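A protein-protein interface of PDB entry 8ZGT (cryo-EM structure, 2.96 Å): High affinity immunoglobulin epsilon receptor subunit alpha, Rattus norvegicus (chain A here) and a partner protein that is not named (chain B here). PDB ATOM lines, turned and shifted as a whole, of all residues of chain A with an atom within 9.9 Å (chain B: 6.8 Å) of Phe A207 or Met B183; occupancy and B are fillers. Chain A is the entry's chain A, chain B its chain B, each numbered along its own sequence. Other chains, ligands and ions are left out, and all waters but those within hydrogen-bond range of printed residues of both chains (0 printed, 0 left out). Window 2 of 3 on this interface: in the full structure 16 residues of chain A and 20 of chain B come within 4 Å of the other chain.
OE1 of Gln A204 sits close to OE2 of Glu B179.
Among the printed residues, merely in contact across the chains: Leu A203 with Phe B176, Gln A204 with Phe B176, Phe A207 with Phe B176, Phe A207 with Met B183, Phe A207 with Leu B180 and Phe A207 with Glu B179.
Of the printed residues of chain B, Leu A203 touches Phe B176. Printed residues of chain B within 4 Å of Phe A207: Phe B176 (3.5 Å), Glu B179 (3.99 Å), Leu B180 (3.7 Å) and Met B183 (3.6 Å). Printed residues of chain A within 4 Å of Phe B176: Leu A203, Gln A204 and Phe A207. Of the printed residues of chain A, Glu B179 touches Gln A204 and Phe A207. Of chain A, only Phe A207 comes within 4 Å of Leu B180. No residue of chain A comes within 4 Å of Leu B182. Of chain A, only Phe A207 (3.6 Å) comes within 4 Å of Met B183. No residue of chain A comes within 4 Å of Leu B184. The nearest printed residue of chain B that does not touch Phe A207 is Phe B75 (4.1 Å). The nearest printed residue of chain B that does not touch Leu A203 is Leu B180 (7.3 Å).
Hydrophobic or aromatic side chains of chain B within 4 Å of the printed part of chain A: Phe B176, Leu B180 and Met B183. Along chain B the printed residues that touch a printed residue of chain A span positions 176 to 183. Among the printed residues, 7 pairs touch across the chains.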
ATOM      1  N   ARG A 201      -2.313   6.863  23.829  1.00  0.00           N
ATOM      2  CA  ARG A 201      -3.174   7.745  24.605  1.00  0.00           C
ATOM      3  C   ARG A 201      -2.570   9.126  24.814  1.00  0.00           C
ATOM      4  O   ARG A 201      -3.315  10.078  25.064  1.00  0.00           O
ATOM      5  CB  ARG A 201      -3.488   7.111  25.961  1.00  0.00           C
ATOM      6  CG  ARG A 201      -4.380   5.884  25.892  1.00  0.00           C
ATOM      7  CD  ARG A 201      -5.841   6.249  26.099  1.00  0.00           C
ATOM      8  NE  ARG A 201      -6.729   5.172  25.682  1.00  0.00           N
ATOM      9  CZ  ARG A 201      -8.052   5.223  25.737  1.00  0.00           C
ATOM     10  NH1 ARG A 201      -8.684   6.303  26.168  1.00  0.00           N
ATOM     11  NH2 ARG A 201      -8.759   4.166  25.352  1.00  0.00           N
ATOM     12  N   TRP A 202      -1.247   9.262  24.711  1.00  0.00           N
ATOM     13  CA  TRP A 202      -0.614  10.564  24.879  1.00  0.00           C
ATOM     14  C   TRP A 202      -0.801  11.475  23.675  1.00  0.00           C
ATOM     15  O   TRP A 202      -0.490  12.666  23.772  1.00  0.00           O
ATOM     16  CB  TRP A 202       0.883  10.403  25.164  1.00  0.00           C
ATOM     17  CG  TRP A 202       1.695   9.872  24.013  1.00  0.00           C
ATOM     18  CD1 TRP A 202       2.306  10.602  23.029  1.00  0.00           C
ATOM     19  CD2 TRP A 202       2.004   8.503  23.744  1.00  0.00           C
ATOM     20  NE1 TRP A 202       2.961   9.767  22.158  1.00  0.00           N
ATOM     21  CE2 TRP A 202       2.793   8.473  22.576  1.00  0.00           C
ATOM     22  CE3 TRP A 202       1.686   7.297  24.373  1.00  0.00           C
ATOM     23  CZ2 TRP A 202       3.267   7.287  22.028  1.00  0.00           C
ATOM     24  CZ3 TRP A 202       2.159   6.122  23.829  1.00  0.00           C
ATOM     25  CH2 TRP A 202       2.941   6.124  22.667  1.00  0.00           C
ATOM     26  N   LEU A 203      -1.278  10.944  22.545  1.00  0.00           N
ATOM     27  CA  LEU A 203      -1.473  11.759  21.354  1.00  0.00           C
ATOM     28  C   LEU A 203      -2.607  12.760  21.515  1.00  0.00           C
ATOM     29  O   LEU A 203      -2.608  13.788  20.835  1.00  0.00           O
ATOM     30  CB  LEU A 203      -1.742  10.866  20.141  1.00  0.00           C
ATOM     31  CG  LEU A 203      -0.558  10.421  19.281  1.00  0.00           C
ATOM     32  CD1 LEU A 203      -1.042  10.052  17.892  1.00  0.00           C
ATOM     33  CD2 LEU A 203       0.521  11.491  19.201  1.00  0.00           C
ATOM     34  N   GLN A 204      -3.564  12.488  22.398  1.00  0.00           N
ATOM     35  CA  GLN A 204      -4.651  13.424  22.642  1.00  0.00           C
ATOM     36  C   GLN A 204      -4.294  14.471  23.690  1.00  0.00           C
ATOM     37  O   GLN A 204      -5.116  15.347  23.975  1.00  0.00           O
ATOM     38  CB  GLN A 204      -5.909  12.664  23.065  1.00  0.00           C
ATOM     39  CG  GLN A 204      -7.202  13.250  22.519  1.00  0.00           C
ATOM     40  CD  GLN A 204      -7.434  12.914  21.057  1.00  0.00           C
ATOM     41  OE1 GLN A 204      -7.017  13.654  20.166  1.00  0.00           O
ATOM     42  NE2 GLN A 204      -8.087  11.787  20.803  1.00  0.00           N
ATOM     43  N   LEU A 205      -3.089  14.403  24.261  1.00  0.00           N
ATOM     44  CA  LEU A 205      -2.597  15.397  25.206  1.00  0.00           C
ATOM     45  C   LEU A 205      -1.803  16.503  24.525  1.00  0.00           C
ATOM     46  O   LEU A 205      -0.901  17.086  25.142  1.00  0.00           O
ATOM     47  CB  LEU A 205      -1.748  14.721  26.283  1.00  0.00           C
ATOM     48  CG  LEU A 205      -2.506  13.982  27.387  1.00  0.00           C
ATOM     49  CD1 LEU A 205      -1.565  13.088  28.177  1.00  0.00           C
ATOM     50  CD2 LEU A 205      -3.212  14.967  28.306  1.00  0.00           C
ATOM     51  N   ILE A 206      -2.109  16.800  23.266  1.00  0.00           N
ATOM     52  CA  ILE A 206      -1.404  17.825  22.509  1.00  0.00           C
ATOM     53  C   ILE A 206      -2.124  19.167  22.575  1.00  0.00           C
ATOM     54  O   ILE A 206      -1.501  20.196  22.836  1.00  0.00           O
ATOM     55  CB  ILE A 206      -1.218  17.356  21.048  1.00  0.00           C
ATOM     56  CG1 ILE A 206      -0.263  16.158  20.971  1.00  0.00           C
ATOM     57  CG2 ILE A 206      -0.699  18.482  20.165  1.00  0.00           C
ATOM     58  CD1 ILE A 206       0.987  16.278  21.829  1.00  0.00           C
ATOM     59  N   PHE A 207      -3.439  19.167  22.351  1.00  0.00           N
ATOM     60  CA  PHE A 207      -4.254  20.381  22.327  1.00  0.00           C
ATOM     61  C   PHE A 207      -4.333  21.121  23.671  1.00  0.00           C
ATOM     62  O   PHE A 207      -4.250  22.357  23.655  1.00  0.00           O
ATOM     63  CB  PHE A 207      -5.655  20.066  21.782  1.00  0.00           C
ATOM     64  CG  PHE A 207      -5.654  19.087  20.642  1.00  0.00           C
ATOM     65  CD1 PHE A 207      -4.937  19.349  19.481  1.00  0.00           C
ATOM     66  CD2 PHE A 207      -6.374  17.905  20.727  1.00  0.00           C
ATOM     67  CE1 PHE A 207      -4.929  18.444  18.434  1.00  0.00           C
ATOM     68  CE2 PHE A 207      -6.377  17.000  19.678  1.00  0.00           C
ATOM     69  CZ  PHE A 207      -5.656  17.271  18.532  1.00  0.00           C
ATOM     70  N   PRO A 208      -4.511  20.469  24.840  1.00  0.00           N
ATOM     71  CA  PRO A 208      -4.291  21.221  26.090  1.00  0.00           C
ATOM     72  C   PRO A 208      -2.856  21.682  26.272  1.00  0.00           C
ATOM     73  O   PRO A 208      -2.625  22.777  26.803  1.00  0.00           O
ATOM     74  CB  PRO A 208      -4.709  20.224  27.180  1.00  0.00           C
ATOM     75  CG  PRO A 208      -4.548  18.905  26.553  1.00  0.00           C
ATOM     76  CD  PRO A 208      -5.037  19.126  25.164  1.00  0.00           C
ATOM     77  N   SER A 209      -1.882  20.892  25.809  1.00  0.00           N
ATOM     78  CA  SER A 209      -0.486  21.307  25.865  1.00  0.00           C
ATOM     79  C   SER A 209      -0.182  22.442  24.897  1.00  0.00           C
ATOM     80  O   SER A 209       0.850  23.101  25.044  1.00  0.00           O
ATOM     81  CB  SER A 209       0.429  20.119  25.576  1.00  0.00           C
ATOM     82  OG  SER A 209       1.740  20.556  25.265  1.00  0.00           O
ATOM     83  N   LEU A 210      -1.044  22.672  23.907  1.00  0.00           N
ATOM     84  CA  LEU A 210      -0.961  23.853  23.061  1.00  0.00           C
ATOM     85  C   LEU A 210      -1.700  25.042  23.663  1.00  0.00           C
ATOM     86  O   LEU A 210      -1.273  26.192  23.484  1.00  0.00           O
ATOM     87  CB  LEU A 210      -1.522  23.526  21.673  1.00  0.00           C
ATOM     88  CG  LEU A 210      -1.531  24.593  20.580  1.00  0.00           C
ATOM     89  CD1 LEU A 210      -0.120  25.034  20.260  1.00  0.00           C
ATOM     90  CD2 LEU A 210      -2.207  24.046  19.342  1.00  0.00           C
ATOM     91  N   ALA A 211      -2.793  24.783  24.388  1.00  0.00           N
ATOM     92  CA  ALA A 211      -3.523  25.854  25.060  1.00  0.00           C
ATOM     93  C   ALA A 211      -2.704  26.470  26.190  1.00  0.00           C
ATOM     94  O   ALA A 211      -2.772  27.684  26.420  1.00  0.00           O
ATOM     95  CB  ALA A 211      -4.857  25.328  25.588  1.00  0.00           C
ATOM     96  N   VAL A 212      -1.918  25.655  26.902  1.00  0.00           N
ATOM     97  CA  VAL A 212      -1.054  26.211  27.946  1.00  0.00           C
ATOM     98  C   VAL A 212       0.133  26.987  27.377  1.00  0.00           C
ATOM     99  O   VAL A 212       0.778  27.740  28.115  1.00  0.00           O
ATOM    100  CB  VAL A 212      -0.556  25.128  28.924  1.00  0.00           C
ATOM    101  CG1 VAL A 212      -1.719  24.341  29.496  1.00  0.00           C
ATOM    102  CG2 VAL A 212       0.431  24.198  28.238  1.00  0.00           C
ATOM    103  N   ILE A 213       0.448  26.828  26.089  1.00  0.00           N
ATOM    104  CA  ILE A 213       1.429  27.708  25.461  1.00  0.00           C
ATOM    105  C   ILE A 213       0.760  28.986  24.970  1.00  0.00           C
ATOM    106  O   ILE A 213       1.316  30.084  25.110  1.00  0.00           O
ATOM    107  CB  ILE A 213       2.159  26.970  24.322  1.00  0.00           C
ATOM    108  CG1 ILE A 213       2.809  25.693  24.844  1.00  0.00           C
ATOM    109  CG2 ILE A 213       3.221  27.855  23.682  1.00  0.00           C
ATOM    110  CD1 ILE A 213       3.427  24.837  23.759  1.00  0.00           C
ATOM    111  N   LEU A 214      -0.446  28.861  24.404  1.00  0.00           N
ATOM    112  CA  LEU A 214      -1.147  30.024  23.861  1.00  0.00           C
ATOM    113  C   LEU A 214      -1.568  30.999  24.959  1.00  0.00           C
ATOM    114  O   LEU A 214      -1.477  32.220  24.779  1.00  0.00           O
ATOM    115  CB  LEU A 214      -2.361  29.570  23.048  1.00  0.00           C
ATOM    116  CG  LEU A 214      -2.223  29.486  21.522  1.00  0.00           C
ATOM    117  CD1 LEU A 214      -3.579  29.651  20.861  1.00  0.00           C
ATOM    118  CD2 LEU A 214      -1.234  30.506  20.966  1.00  0.00           C
ATOM    119  N   PHE A 215      -2.008  30.485  26.112  1.00  0.00           N
ATOM    120  CA  PHE A 215      -2.379  31.373  27.211  1.00  0.00           C
ATOM    121  C   PHE A 215      -1.157  32.026  27.849  1.00  0.00           C
ATOM    122  O   PHE A 215      -1.239  33.174  28.308  1.00  0.00           O
ATOM    123  CB  PHE A 215      -3.188  30.603  28.253  1.00  0.00           C
ATOM    124  CG  PHE A 215      -4.587  30.270  27.808  1.00  0.00           C
ATOM    125  CD1 PHE A 215      -5.223  31.030  26.837  1.00  0.00           C
ATOM    126  CD2 PHE A 215      -5.265  29.198  28.363  1.00  0.00           C
ATOM    127  CE1 PHE A 215      -6.511  30.721  26.427  1.00  0.00           C
ATOM    128  CE2 PHE A 215      -6.550  28.884  27.958  1.00  0.00           C
ATOM    129  CZ  PHE A 215      -7.174  29.648  26.990  1.00  0.00           C
ATOM    130  N   ILE B  71       1.479  27.180  13.741  1.00  0.00           N
ATOM    131  CA  ILE B  71       0.647  26.091  14.247  1.00  0.00           C
ATOM    132  C   ILE B  71       0.654  24.910  13.275  1.00  0.00           C
ATOM    133  O   ILE B  71       0.671  23.747  13.698  1.00  0.00           O
ATOM    134  CB  ILE B  71      -0.770  26.616  14.550  1.00  0.00           C
ATOM    135  CG1 ILE B  71      -0.716  27.531  15.775  1.00  0.00           C
ATOM    136  CG2 ILE B  71      -1.761  25.486  14.815  1.00  0.00           C
ATOM    137  CD1 ILE B  71      -2.053  28.022  16.248  1.00  0.00           C
ATOM    138  N   PHE B  75       1.982  21.260  14.261  1.00  0.00           N
ATOM    139  CA  PHE B  75       1.147  20.086  14.032  1.00  0.00           C
ATOM    140  C   PHE B  75       1.850  19.053  13.161  1.00  0.00           C
ATOM    141  O   PHE B  75       1.664  17.849  13.365  1.00  0.00           O
ATOM    142  CB  PHE B  75      -0.178  20.501  13.395  1.00  0.00           C
ATOM    143  CG  PHE B  75      -1.235  20.890  14.388  1.00  0.00           C
ATOM    144  CD1 PHE B  75      -1.186  20.431  15.694  1.00  0.00           C
ATOM    145  CD2 PHE B  75      -2.286  21.713  14.013  1.00  0.00           C
ATOM    146  CE1 PHE B  75      -2.159  20.788  16.607  1.00  0.00           C
ATOM    147  CE2 PHE B  75      -3.263  22.072  14.920  1.00  0.00           C
ATOM    148  CZ  PHE B  75      -3.199  21.609  16.218  1.00  0.00           C
ATOM    149  N   LEU B 148      -7.113  18.715   2.339  1.00  0.00           N
ATOM    150  CA  LEU B 148      -7.764  18.420   3.610  1.00  0.00           C
ATOM    151  C   LEU B 148      -9.193  17.923   3.415  1.00  0.00           C
ATOM    152  O   LEU B 148      -9.666  17.104   4.208  1.00  0.00           O
ATOM    153  CB  LEU B 148      -7.742  19.658   4.507  1.00  0.00           C
ATOM    154  CG  LEU B 148      -6.405  19.965   5.187  1.00  0.00           C
ATOM    155  CD1 LEU B 148      -6.457  21.298   5.911  1.00  0.00           C
ATOM    156  CD2 LEU B 148      -6.007  18.854   6.133  1.00  0.00           C
ATOM    157  N   PHE B 176      -7.865  10.979  15.682  1.00  0.00           N
ATOM    158  CA  PHE B 176      -6.953  12.073  16.020  1.00  0.00           C
ATOM    159  C   PHE B 176      -6.544  12.860  14.779  1.00  0.00           C
ATOM    160  O   PHE B 176      -6.480  14.099  14.805  1.00  0.00           O
ATOM    161  CB  PHE B 176      -5.727  11.509  16.740  1.00  0.00           C
ATOM    162  CG  PHE B 176      -4.588  12.480  16.863  1.00  0.00           C
ATOM    163  CD1 PHE B 176      -4.676  13.566  17.720  1.00  0.00           C
ATOM    164  CD2 PHE B 176      -3.422  12.299  16.132  1.00  0.00           C
ATOM    165  CE1 PHE B 176      -3.627  14.459  17.836  1.00  0.00           C
ATOM    166  CE2 PHE B 176      -2.371  13.189  16.244  1.00  0.00           C
ATOM    167  CZ  PHE B 176      -2.475  14.270  17.097  1.00  0.00           C
ATOM    168  N   THR B 178      -8.426  13.107  12.195  1.00  0.00           N
ATOM    169  CA  THR B 178      -9.636  13.840  11.819  1.00  0.00           C
ATOM    170  C   THR B 178      -9.757  15.169  12.565  1.00  0.00           C
ATOM    171  O   THR B 178     -10.118  16.189  11.960  1.00  0.00           O
ATOM    172  CB  THR B 178     -10.870  12.970  12.063  1.00  0.00           C
ATOM    173  OG1 THR B 178     -10.682  11.691  11.445  1.00  0.00           O
ATOM    174  CG2 THR B 178     -12.117  13.620  11.493  1.00  0.00           C
ATOM    175  N   GLU B 179      -9.463  15.182  13.876  1.00  0.00           N
ATOM    176  CA  GLU B 179      -9.427  16.464  14.595  1.00  0.00           C
ATOM    177  C   GLU B 179      -8.326  17.377  14.063  1.00  0.00           C
ATOM    178  O   GLU B 179      -8.523  18.598  13.952  1.00  0.00           O
ATOM    179  CB  GLU B 179      -9.247  16.288  16.105  1.00  0.00           C
ATOM    180  CG  GLU B 179      -9.785  15.031  16.720  1.00  0.00           C
ATOM    181  CD  GLU B 179     -10.053  15.177  18.204  1.00  0.00           C
ATOM    182  OE1 GLU B 179     -10.178  16.327  18.675  1.00  0.00           O
ATOM    183  OE2 GLU B 179     -10.131  14.142  18.898  1.00  0.00           O
ATOM    184  N   LEU B 180      -7.163  16.804  13.728  1.00  0.00           N
ATOM    185  CA  LEU B 180      -6.083  17.594  13.135  1.00  0.00           C
ATOM    186  C   LEU B 180      -6.495  18.185  11.790  1.00  0.00           C
ATOM    187  O   LEU B 180      -6.193  19.346  11.499  1.00  0.00           O
ATOM    188  CB  LEU B 180      -4.830  16.734  12.978  1.00  0.00           C
ATOM    189  CG  LEU B 180      -3.838  16.642  14.140  1.00  0.00           C
ATOM    190  CD1 LEU B 180      -2.459  16.295  13.612  1.00  0.00           C
ATOM    191  CD2 LEU B 180      -3.788  17.927  14.951  1.00  0.00           C
ATOM    192  N   VAL B 181      -7.217  17.410  10.979  1.00  0.00           N
ATOM    193  CA  VAL B 181      -7.705  17.878   9.684  1.00  0.00           C
ATOM    194  C   VAL B 181      -8.717  19.006   9.864  1.00  0.00           C
ATOM    195  O   VAL B 181      -8.674  20.010   9.144  1.00  0.00           O
ATOM    196  CB  VAL B 181      -8.282  16.688   8.889  1.00  0.00           C
ATOM    197  CG1 VAL B 181      -9.333  17.122   7.869  1.00  0.00           C
ATOM    198  CG2 VAL B 181      -7.167  15.929   8.191  1.00  0.00           C
ATOM    199  N   LEU B 182      -9.605  18.884  10.857  1.00  0.00           N
ATOM    200  CA  LEU B 182     -10.636  19.901  11.073  1.00  0.00           C
ATOM    201  C   LEU B 182     -10.043  21.232  11.541  1.00  0.00           C
ATOM    202  O   LEU B 182     -10.356  22.295  10.980  1.00  0.00           O
ATOM    203  CB  LEU B 182     -11.670  19.388  12.074  1.00  0.00           C
ATOM    204  CG  LEU B 182     -12.737  18.459  11.493  1.00  0.00           C
ATOM    205  CD1 LEU B 182     -13.337  17.578  12.574  1.00  0.00           C
ATOM    206  CD2 LEU B 182     -13.820  19.263  10.793  1.00  0.00           C
ATOM    207  N   MET B 183      -9.169  21.200  12.548  1.00  0.00           N
ATOM    208  CA  MET B 183      -8.564  22.455  12.992  1.00  0.00           C
ATOM    209  C   MET B 183      -7.308  22.842  12.218  1.00  0.00           C
ATOM    210  O   MET B 183      -6.640  23.807  12.603  1.00  0.00           O
ATOM    211  CB  MET B 183      -8.282  22.440  14.500  1.00  0.00           C
ATOM    212  CG  MET B 183      -9.117  21.458  15.284  1.00  0.00           C
ATOM    213  SD  MET B 183      -8.955  21.662  17.063  1.00  0.00           S
ATOM    214  CE  MET B 183      -7.787  20.368  17.435  1.00  0.00           C
ATOM    215  N   LEU B 184      -6.963  22.127  11.148  1.00  0.00           N
ATOM    216  CA  LEU B 184      -6.136  22.730  10.113  1.00  0.00           C
ATOM    217  C   LEU B 184      -6.972  23.364   9.013  1.00  0.00           C
ATOM    218  O   LEU B 184      -6.558  24.376   8.437  1.00  0.00           O
ATOM    219  CB  LEU B 184      -5.182  21.698   9.503  1.00  0.00           C
ATOM    220  CG  LEU B 184      -3.915  21.382  10.300  1.00  0.00           C
ATOM    221  CD1 LEU B 184      -3.037  20.391   9.558  1.00  0.00           C
ATOM    222  CD2 LEU B 184      -3.155  22.651  10.606  1.00  0.00           C
ATOM    223  N   LEU B 185      -8.153  22.802   8.730  1.00  0.00           N
ATOM    224  CA  LEU B 185      -9.047  23.364   7.723  1.00  0.00           C
ATOM    225  C   LEU B 185      -9.601  24.715   8.158  1.00  0.00           C
ATOM    226  O   LEU B 185      -9.738  25.623   7.330  1.00  0.00           O
ATOM    227  CB  LEU B 185     -10.190  22.389   7.440  1.00  0.00           C
ATOM    228  CG  LEU B 185     -11.096  22.625   6.226  1.00  0.00           C
ATOM    229  CD1 LEU B 185     -10.316  23.147   5.028  1.00  0.00           C
ATOM    230  CD2 LEU B 185     -11.841  21.348   5.869  1.00  0.00           C
ATOM    231  N   PHE B 186      -9.926  24.857   9.449  1.00  0.00           N
ATOM    232  CA  PHE B 186     -10.432  26.134   9.960  1.00  0.00           C
ATOM    233  C   PHE B 186      -9.387  27.245   9.832  1.00  0.00           C
ATOM    234  O   PHE B 186      -9.682  28.346   9.341  1.00  0.00           O
ATOM    235  CB  PHE B 186     -10.872  25.967  11.415  1.00  0.00           C
ATOM    236  CG  PHE B 186     -11.180  27.262  12.114  1.00  0.00           C
ATOM    237  CD1 PHE B 186     -12.302  28.001  11.772  1.00  0.00           C
ATOM    238  CD2 PHE B 186     -10.355  27.732  13.126  1.00  0.00           C
ATOM    239  CE1 PHE B 186     -12.590  29.193  12.419  1.00  0.00           C
ATOM    240  CE2 PHE B 186     -10.637  28.922  13.777  1.00  0.00           C
ATOM    241  CZ  PHE B 186     -11.756  29.653  13.422  1.00  0.00           C
ATOM    242  N   LEU B 187      -8.147  26.952  10.231  1.00  0.00           N
ATOM    243  CA  LEU B 187      -7.073  27.934  10.122  1.00  0.00           C
ATOM    244  C   LEU B 187      -6.691  28.201   8.672  1.00  0.00           C
ATOM    245  O   LEU B 187      -6.321  29.331   8.336  1.00  0.00           O
ATOM    246  CB  LEU B 187      -5.853  27.466  10.914  1.00  0.00           C
ATOM    247  CG  LEU B 187      -6.047  27.331  12.423  1.00  0.00           C
ATOM    248  CD1 LEU B 187      -4.852  26.642  13.041  1.00  0.00           C
ATOM    249  CD2 LEU B 187      -6.270  28.690  13.059  1.00  0.00           C
ATOM    250  N   THR B 188      -6.781  27.190   7.801  1.00  0.00           N
ATOM    251  CA  THR B 188      -6.503  27.400   6.384  1.00  0.00           C
ATOM    252  C   THR B 188      -7.555  28.294   5.738  1.00  0.00           C
ATOM    253  O   THR B 188      -7.215  29.150   4.916  1.00  0.00           O
ATOM    254  CB  THR B 188      -6.424  26.058   5.659  1.00  0.00           C
ATOM    255  OG1 THR B 188      -5.616  25.152   6.419  1.00  0.00           O
ATOM    256  CG2 THR B 188      -5.807  26.235   4.282  1.00  0.00           C
